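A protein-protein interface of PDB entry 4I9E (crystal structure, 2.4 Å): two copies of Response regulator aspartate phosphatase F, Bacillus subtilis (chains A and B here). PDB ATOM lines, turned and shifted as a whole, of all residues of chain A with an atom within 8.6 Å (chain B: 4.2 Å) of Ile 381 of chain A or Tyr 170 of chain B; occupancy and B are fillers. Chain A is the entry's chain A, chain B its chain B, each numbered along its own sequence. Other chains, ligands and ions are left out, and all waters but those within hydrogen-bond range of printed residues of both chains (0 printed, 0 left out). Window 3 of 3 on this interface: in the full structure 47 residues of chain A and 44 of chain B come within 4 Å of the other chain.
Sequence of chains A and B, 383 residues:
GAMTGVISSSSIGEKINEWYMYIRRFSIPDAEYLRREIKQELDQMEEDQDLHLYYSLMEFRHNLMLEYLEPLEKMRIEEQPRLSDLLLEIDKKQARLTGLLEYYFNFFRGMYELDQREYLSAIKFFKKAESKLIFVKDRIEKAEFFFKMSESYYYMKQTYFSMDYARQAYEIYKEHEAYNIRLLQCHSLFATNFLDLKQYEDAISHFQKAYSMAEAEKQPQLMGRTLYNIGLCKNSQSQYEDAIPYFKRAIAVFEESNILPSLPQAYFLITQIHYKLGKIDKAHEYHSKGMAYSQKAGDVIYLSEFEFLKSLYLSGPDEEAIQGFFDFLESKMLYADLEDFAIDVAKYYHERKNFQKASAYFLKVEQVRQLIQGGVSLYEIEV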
ATOM      1  N   LEU A 120     -12.045  -7.185  11.606  1.00  0.00           N
ATOM      2  CA  LEU A 120     -12.361  -6.119  12.531  1.00  0.00           C
ATOM      3  C   LEU A 120     -13.855  -6.142  12.789  1.00  0.00           C
ATOM      4  O   LEU A 120     -14.327  -5.990  13.926  1.00  0.00           O
ATOM      5  CB  LEU A 120     -11.908  -4.792  11.935  1.00  0.00           C
ATOM      6  CG  LEU A 120     -10.396  -4.516  11.908  1.00  0.00           C
ATOM      7  CD1 LEU A 120     -10.098  -3.019  11.539  1.00  0.00           C
ATOM      8  CD2 LEU A 120      -9.696  -4.892  13.219  1.00  0.00           C
ATOM      9  N   SER A 377     -10.239  -3.469   6.813  1.00  0.00           N
ATOM     10  CA  SER A 377     -10.916  -2.239   6.420  1.00  0.00           C
ATOM     11  C   SER A 377     -11.445  -1.570   7.652  1.00  0.00           C
ATOM     12  O   SER A 377     -12.026  -2.205   8.534  1.00  0.00           O
ATOM     13  CB  SER A 377     -12.104  -2.567   5.523  1.00  0.00           C
ATOM     14  OG  SER A 377     -11.687  -3.424   4.463  1.00  0.00           O
ATOM     15  N   LEU A 378     -11.277  -0.277   7.705  1.00  0.00           N
ATOM     16  CA  LEU A 378     -11.948   0.498   8.711  1.00  0.00           C
ATOM     17  C   LEU A 378     -13.435   0.714   8.359  1.00  0.00           C
ATOM     18  O   LEU A 378     -13.822   1.039   7.215  1.00  0.00           O
ATOM     19  CB  LEU A 378     -11.223   1.812   8.883  1.00  0.00           C
ATOM     20  CG  LEU A 378     -10.300   1.931  10.102  1.00  0.00           C
ATOM     21  CD1 LEU A 378     -10.056   0.679  10.982  1.00  0.00           C
ATOM     22  CD2 LEU A 378      -9.018   2.581   9.697  1.00  0.00           C
ATOM     23  N   TYR A 379     -14.260   0.491   9.365  1.00  0.00           N
ATOM     24  CA  TYR A 379     -15.674   0.723   9.300  1.00  0.00           C
ATOM     25  C   TYR A 379     -15.879   2.213   9.524  1.00  0.00           C
ATOM     26  O   TYR A 379     -15.628   2.702  10.620  1.00  0.00           O
ATOM     27  CB  TYR A 379     -16.365  -0.065  10.415  1.00  0.00           C
ATOM     28  CG  TYR A 379     -17.854   0.135  10.447  1.00  0.00           C
ATOM     29  CD1 TYR A 379     -18.463   0.903  11.455  1.00  0.00           C
ATOM     30  CD2 TYR A 379     -18.673  -0.418   9.453  1.00  0.00           C
ATOM     31  CE1 TYR A 379     -19.870   1.100  11.457  1.00  0.00           C
ATOM     32  CE2 TYR A 379     -20.063  -0.223   9.459  1.00  0.00           C
ATOM     33  CZ  TYR A 379     -20.648   0.531  10.456  1.00  0.00           C
ATOM     34  OH  TYR A 379     -22.013   0.719  10.424  1.00  0.00           O
ATOM     35  N   GLU A 380     -16.262   2.935   8.466  1.00  0.00           N
ATOM     36  CA  GLU A 380     -16.703   4.328   8.585  1.00  0.00           C
ATOM     37  C   GLU A 380     -15.690   5.340   9.092  1.00  0.00           C
ATOM     38  O   GLU A 380     -16.037   6.267   9.796  1.00  0.00           O
ATOM     39  CB  GLU A 380     -17.934   4.399   9.485  1.00  0.00           C
ATOM     40  CG  GLU A 380     -19.164   3.709   8.919  1.00  0.00           C
ATOM     41  CD  GLU A 380     -20.387   4.072   9.720  1.00  0.00           C
ATOM     42  OE1 GLU A 380     -20.208   4.754  10.763  1.00  0.00           O
ATOM     43  OE2 GLU A 380     -21.513   3.692   9.312  1.00  0.00           O
ATOM     44  N   ILE A 381     -14.432   5.182   8.747  1.00  0.00           N
ATOM     45  CA  ILE A 381     -13.471   6.169   9.186  1.00  0.00           C
ATOM     46  C   ILE A 381     -12.856   6.855   7.978  1.00  0.00           C
ATOM     47  O   ILE A 381     -12.350   6.196   7.064  1.00  0.00           O
ATOM     48  CB  ILE A 381     -12.448   5.578  10.187  1.00  0.00           C
ATOM     49  CG1 ILE A 381     -13.236   5.056  11.422  1.00  0.00           C
ATOM     50  CG2 ILE A 381     -11.341   6.596  10.491  1.00  0.00           C
ATOM     51  CD1 ILE A 381     -12.503   4.935  12.730  1.00  0.00           C
ATOM     52  N   GLU A 382     -12.936   8.182   7.969  1.00  0.00           N
ATOM     53  CA  GLU A 382     -12.552   8.967   6.811  1.00  0.00           C
ATOM     54  C   GLU A 382     -11.128   9.513   6.904  1.00  0.00           C
ATOM     55  O   GLU A 382     -10.769  10.211   7.863  1.00  0.00           O
ATOM     56  CB  GLU A 382     -13.562  10.120   6.595  1.00  0.00           C
ATOM     57  N   VAL A 383     -10.318   9.208   5.898  1.00  0.00           N
ATOM     58  CA  VAL A 383      -9.020   9.858   5.802  1.00  0.00           C
ATOM     59  C   VAL A 383      -9.190  11.242   5.141  1.00  0.00           C
ATOM     60  O   VAL A 383      -9.938  12.156   5.582  1.00  0.00           O
ATOM     61  CB  VAL A 383      -8.024   8.979   5.039  1.00  0.00           C
ATOM     62  OXT VAL A 383      -8.560  11.491   4.099  1.00  0.00           O
ATOM     63  N   ALA B 166      -8.494   1.126  18.997  1.00  0.00           N
ATOM     64  CA  ALA B 166      -8.261   2.445  18.388  1.00  0.00           C
ATOM     65  C   ALA B 166      -9.588   3.031  17.848  1.00  0.00           C
ATOM     66  O   ALA B 166      -9.851   4.215  17.978  1.00  0.00           O
ATOM     67  CB  ALA B 166      -7.237   2.338  17.234  1.00  0.00           C
ATOM     68  N   ARG B 167     -10.380   2.184  17.200  1.00  0.00           N
ATOM     69  CA  ARG B 167     -11.694   2.517  16.657  1.00  0.00           C
ATOM     70  C   ARG B 167     -12.667   2.934  17.776  1.00  0.00           C
ATOM     71  O   ARG B 167     -13.353   3.930  17.661  1.00  0.00           O
ATOM     72  CB  ARG B 167     -12.182   1.327  15.824  1.00  0.00           C
ATOM     73  CG  ARG B 167     -13.674   1.058  15.877  1.00  0.00           C
ATOM     74  CD  ARG B 167     -14.065  -0.291  16.491  1.00  0.00           C
ATOM     75  NE  ARG B 167     -15.390  -0.155  17.049  1.00  0.00           N
ATOM     76  CZ  ARG B 167     -16.016  -1.067  17.772  1.00  0.00           C
ATOM     77  NH1 ARG B 167     -15.488  -2.253  18.016  1.00  0.00           N
ATOM     78  NH2 ARG B 167     -17.205  -0.780  18.250  1.00  0.00           N
ATOM     79  N   GLN B 168     -12.676   2.214  18.885  1.00  0.00           N
ATOM     80  CA  GLN B 168     -13.538   2.577  20.004  1.00  0.00           C
ATOM     81  C   GLN B 168     -13.125   3.920  20.641  1.00  0.00           C
ATOM     82  O   GLN B 168     -13.967   4.714  21.035  1.00  0.00           O
ATOM     83  CB  GLN B 168     -13.518   1.465  21.061  1.00  0.00           C
ATOM     84  CG  GLN B 168     -14.120   0.135  20.638  1.00  0.00           C
ATOM     85  CD  GLN B 168     -14.216  -0.789  21.840  1.00  0.00           C
ATOM     86  OE1 GLN B 168     -14.852  -0.454  22.838  1.00  0.00           O
ATOM     87  NE2 GLN B 168     -13.567  -1.910  21.775  1.00  0.00           N
ATOM     88  N   ALA B 169     -11.816   4.136  20.798  1.00  0.00           N
ATOM     89  CA  ALA B 169     -11.288   5.407  21.279  1.00  0.00           C
ATOM     90  C   ALA B 169     -11.667   6.505  20.285  1.00  0.00           C
ATOM     91  O   ALA B 169     -12.192   7.510  20.714  1.00  0.00           O
ATOM     92  CB  ALA B 169      -9.785   5.355  21.513  1.00  0.00           C
ATOM     93  N   TYR B 170     -11.433   6.288  18.990  1.00  0.00           N
ATOM     94  CA  TYR B 170     -11.775   7.231  17.912  1.00  0.00           C
ATOM     95  C   TYR B 170     -13.215   7.761  17.961  1.00  0.00           C
ATOM     96  O   TYR B 170     -13.407   8.976  17.859  1.00  0.00           O
ATOM     97  CB  TYR B 170     -11.496   6.633  16.528  1.00  0.00           C
ATOM     98  CG  TYR B 170     -11.772   7.541  15.352  1.00  0.00           C
ATOM     99  CD1 TYR B 170     -10.761   8.330  14.780  1.00  0.00           C
ATOM    100  CD2 TYR B 170     -13.058   7.620  14.788  1.00  0.00           C
ATOM    101  CE1 TYR B 170     -11.038   9.186  13.692  1.00  0.00           C
ATOM    102  CE2 TYR B 170     -13.334   8.477  13.676  1.00  0.00           C
ATOM    103  CZ  TYR B 170     -12.326   9.265  13.157  1.00  0.00           C
ATOM    104  OH  TYR B 170     -12.621  10.084  12.051  1.00  0.00           O
ATOM    105  N   GLU B 171     -14.187   6.861  18.093  1.00  0.00           N
ATOM    106  CA  GLU B 171     -15.605   7.168  18.176  1.00  0.00           C
ATOM    107  C   GLU B 171     -15.970   8.130  19.261  1.00  0.00           C
ATOM    108  O   GLU B 171     -16.822   8.976  19.053  1.00  0.00           O
ATOM    109  CB  GLU B 171     -16.434   5.910  18.380  1.00  0.00           C
ATOM    110  CG  GLU B 171     -16.511   5.048  17.116  1.00  0.00           C
ATOM    111  CD  GLU B 171     -16.974   3.637  17.430  1.00  0.00           C
ATOM    112  OE1 GLU B 171     -17.399   3.399  18.614  1.00  0.00           O
ATOM    113  OE2 GLU B 171     -16.906   2.793  16.494  1.00  0.00           O
ATOM    114  N   ILE B 172     -15.366   7.977  20.428  1.00  0.00           N
ATOM    115  CA  ILE B 172     -15.573   8.900  21.507  1.00  0.00           C
ATOM    116  C   ILE B 172     -14.862  10.249  21.195  1.00  0.00           C
ATOM    117  O   ILE B 172     -15.533  11.272  21.077  1.00  0.00           O
ATOM    118  CB  ILE B 172     -15.117   8.298  22.828  1.00  0.00           C
ATOM    119  CG1 ILE B 172     -15.937   7.058  23.135  1.00  0.00           C
ATOM    120  CG2 ILE B 172     -15.234   9.333  23.930  1.00  0.00           C
ATOM    121  CD1 ILE B 172     -15.459   6.199  24.376  1.00  0.00           C
ATOM    122  N   TYR B 173     -13.536  10.255  21.014  1.00  0.00           N
ATOM    123  CA  TYR B 173     -12.813  11.482  20.669  1.00  0.00           C
ATOM    124  C   TYR B 173     -13.403  12.296  19.514  1.00  0.00           C
ATOM    125  O   TYR B 173     -13.210  13.513  19.451  1.00  0.00           O
ATOM    126  CB  TYR B 173     -11.303  11.228  20.372  1.00  0.00           C
ATOM    127  CG  TYR B 173     -10.484  10.677  21.521  1.00  0.00           C
ATOM    128  CD1 TYR B 173     -10.481  11.292  22.786  1.00  0.00           C
ATOM    129  CD2 TYR B 173      -9.717   9.511  21.345  1.00  0.00           C
ATOM    130  CE1 TYR B 173      -9.715  10.733  23.849  1.00  0.00           C
ATOM    131  CE2 TYR B 173      -8.962   8.976  22.369  1.00  0.00           C
ATOM    132  CZ  TYR B 173      -8.957   9.575  23.612  1.00  0.00           C
ATOM    133  OH  TYR B 173      -8.193   9.021  24.615  1.00  0.00           O
ATOM    134  N   LYS B 174     -14.047  11.610  18.575  1.00  0.00           N
ATOM    135  CA  LYS B 174     -14.584  12.222  17.366  1.00  0.00           C
ATOM    136  C   LYS B 174     -15.754  13.166  17.712  1.00  0.00           C
ATOM    137  O   LYS B 174     -15.795  14.316  17.262  1.00  0.00           O
ATOM    138  CB  LYS B 174     -14.988  11.125  16.367  1.00  0.00           C
ATOM    139  CG  LYS B 174     -15.971  11.537  15.284  1.00  0.00           C
ATOM    140  CD  LYS B 174     -16.482  10.361  14.435  1.00  0.00           C
ATOM    141  CE  LYS B 174     -17.151   9.206  15.252  1.00  0.00           C
ATOM    142  NZ  LYS B 174     -16.980   7.845  14.539  1.00  0.00           N
ATOM    143  N   LEU B 183      -7.440  12.383  18.499  1.00  0.00           N
ATOM    144  CA  LEU B 183      -7.910  11.872  17.204  1.00  0.00           C
ATOM    145  C   LEU B 183      -6.796  11.578  16.168  1.00  0.00           C
ATOM    146  O   LEU B 183      -6.781  10.481  15.560  1.00  0.00           O
ATOM    147  CB  LEU B 183      -8.977  12.789  16.620  1.00  0.00           C
ATOM    148  CG  LEU B 183     -10.017  11.978  15.860  1.00  0.00           C
ATOM    149  CD1 LEU B 183     -10.973  11.324  16.857  1.00  0.00           C
ATOM    150  CD2 LEU B 183     -10.735  12.891  14.855  1.00  0.00           C
ATOM    151  N   CYS B 186      -5.029   8.528  17.104  1.00  0.00           N
ATOM    152  CA  CYS B 186      -5.766   7.336  16.772  1.00  0.00           C
ATOM    153  C   CYS B 186      -5.445   6.928  15.382  1.00  0.00           C
ATOM    154  O   CYS B 186      -5.354   5.739  15.112  1.00  0.00           O
ATOM    155  CB  CYS B 186      -7.283   7.561  16.904  1.00  0.00           C
ATOM    156  SG  CYS B 186      -7.803   7.664  18.568  1.00  0.00           S
ATOM    157  N   HIS B 187      -5.360   7.922  14.484  1.00  0.00           N
ATOM    158  CA  HIS B 187      -4.970   7.734  13.076  1.00  0.00           C
ATOM    159  C   HIS B 187      -3.570   7.119  12.933  1.00  0.00           C
ATOM    160  O   HIS B 187      -3.390   6.291  12.084  1.00  0.00           O
ATOM    161  CB  HIS B 187      -5.043   9.092  12.318  1.00  0.00           C
ATOM    162  CG  HIS B 187      -6.395   9.399  11.744  1.00  0.00           C
ATOM    163  ND1 HIS B 187      -7.001   8.600  10.789  1.00  0.00           N
ATOM    164  CD2 HIS B 187      -7.249  10.435  11.966  1.00  0.00           C
ATOM    165  CE1 HIS B 187      -8.179   9.112  10.475  1.00  0.00           C
ATOM    166  NE2 HIS B 187      -8.361  10.209  11.195  1.00  0.00           N
ATOM    167  N   PHE B 190      -3.986   3.460  13.626  1.00  0.00           N
ATOM    168  CA  PHE B 190      -4.529   2.685  12.513  1.00  0.00           C
ATOM    169  C   PHE B 190      -3.407   2.501  11.534  1.00  0.00           C
ATOM    170  O   PHE B 190      -3.234   1.421  10.920  1.00  0.00           O
ATOM    171  CB  PHE B 190      -5.684   3.406  11.779  1.00  0.00           C
ATOM    172  CG  PHE B 190      -6.921   3.603  12.595  1.00  0.00           C
ATOM    173  CD1 PHE B 190      -7.547   2.524  13.239  1.00  0.00           C
ATOM    174  CD2 PHE B 190      -7.485   4.874  12.705  1.00  0.00           C
ATOM    175  CE1 PHE B 190      -8.748   2.704  13.966  1.00  0.00           C
ATOM    176  CE2 PHE B 190      -8.665   5.083  13.466  1.00  0.00           C
ATOM    177  CZ  PHE B 190      -9.281   3.988  14.105  1.00  0.00           C
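Hydrophobic or aromatic side chains of chain B within 4 Å of the printed part of chain A: Tyr 170, His 187 and Phe 190. Along chain B the printed residues that touch a printed residue of chain A span positions 170 to 190. Of the 8 printed residues of chain A, 3 touch a printed residue of chain B. Printed residues of chain A that touch a printed residue of chain B: Leu 378, Ile 381 and Glu 382. Hydrophobic or aromatic side chains of chain A within 4 Å of the printed part of chain B: Leu 378 and Ile 381. Among the printed residues, no Asp or Glu carboxylate lies within 4 Å of a Lys or Arg side-chain nitrogen of the other chain.
No position is printed for both chains. Of the 4 pairs that touch across the chains among the printed residues, none has its exchanged pair printed and touching as well.
Of the printed residues of chain B, Leu 378 of chain A touches Phe 190 (3.7 Å). Ile 381 of chain A touches just these residues of chain B: Tyr 170 (3.4 Å) and Phe 190 (3.6 Å). Of the printed residues of chain B, Glu 382 of chain A touches His 187 (3.8 Å). Of chain A, only Ile 381 comes within 4 Å of Tyr 170 of chain B. Glu 171 of chain B touches none of the printed residues of chain A. Lys 174 of chain B touches none of the printed residues of chain A. Printed residues of chain A within 4 Å of His 187 of chain B: Glu 382. Of the printed residues of chain A, Phe 190 of chain B touches Leu 378 and Ile 381. The nearest residue of chain B that does not touch Ile 381 of chain A is His 187 of chain B (4.04 Å). The nearest residue of chain A that does not touch Tyr 170 of chain B is Glu 382 of chain A (4.5 Å). The nearest printed residue of chain B that does not touch Glu 382 of chain A is Tyr 170 of chain B (4.5 Å).
Among the printed residues, pairs that only touch across the chains: Ile 381 of chain A with Tyr 170 of chain B, Ile 381 of chain A with Phe 190 of chain B, Leu 378 of chain A with Phe 190 of chain B and Glu 382 of chain A with His 187 of chain B.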
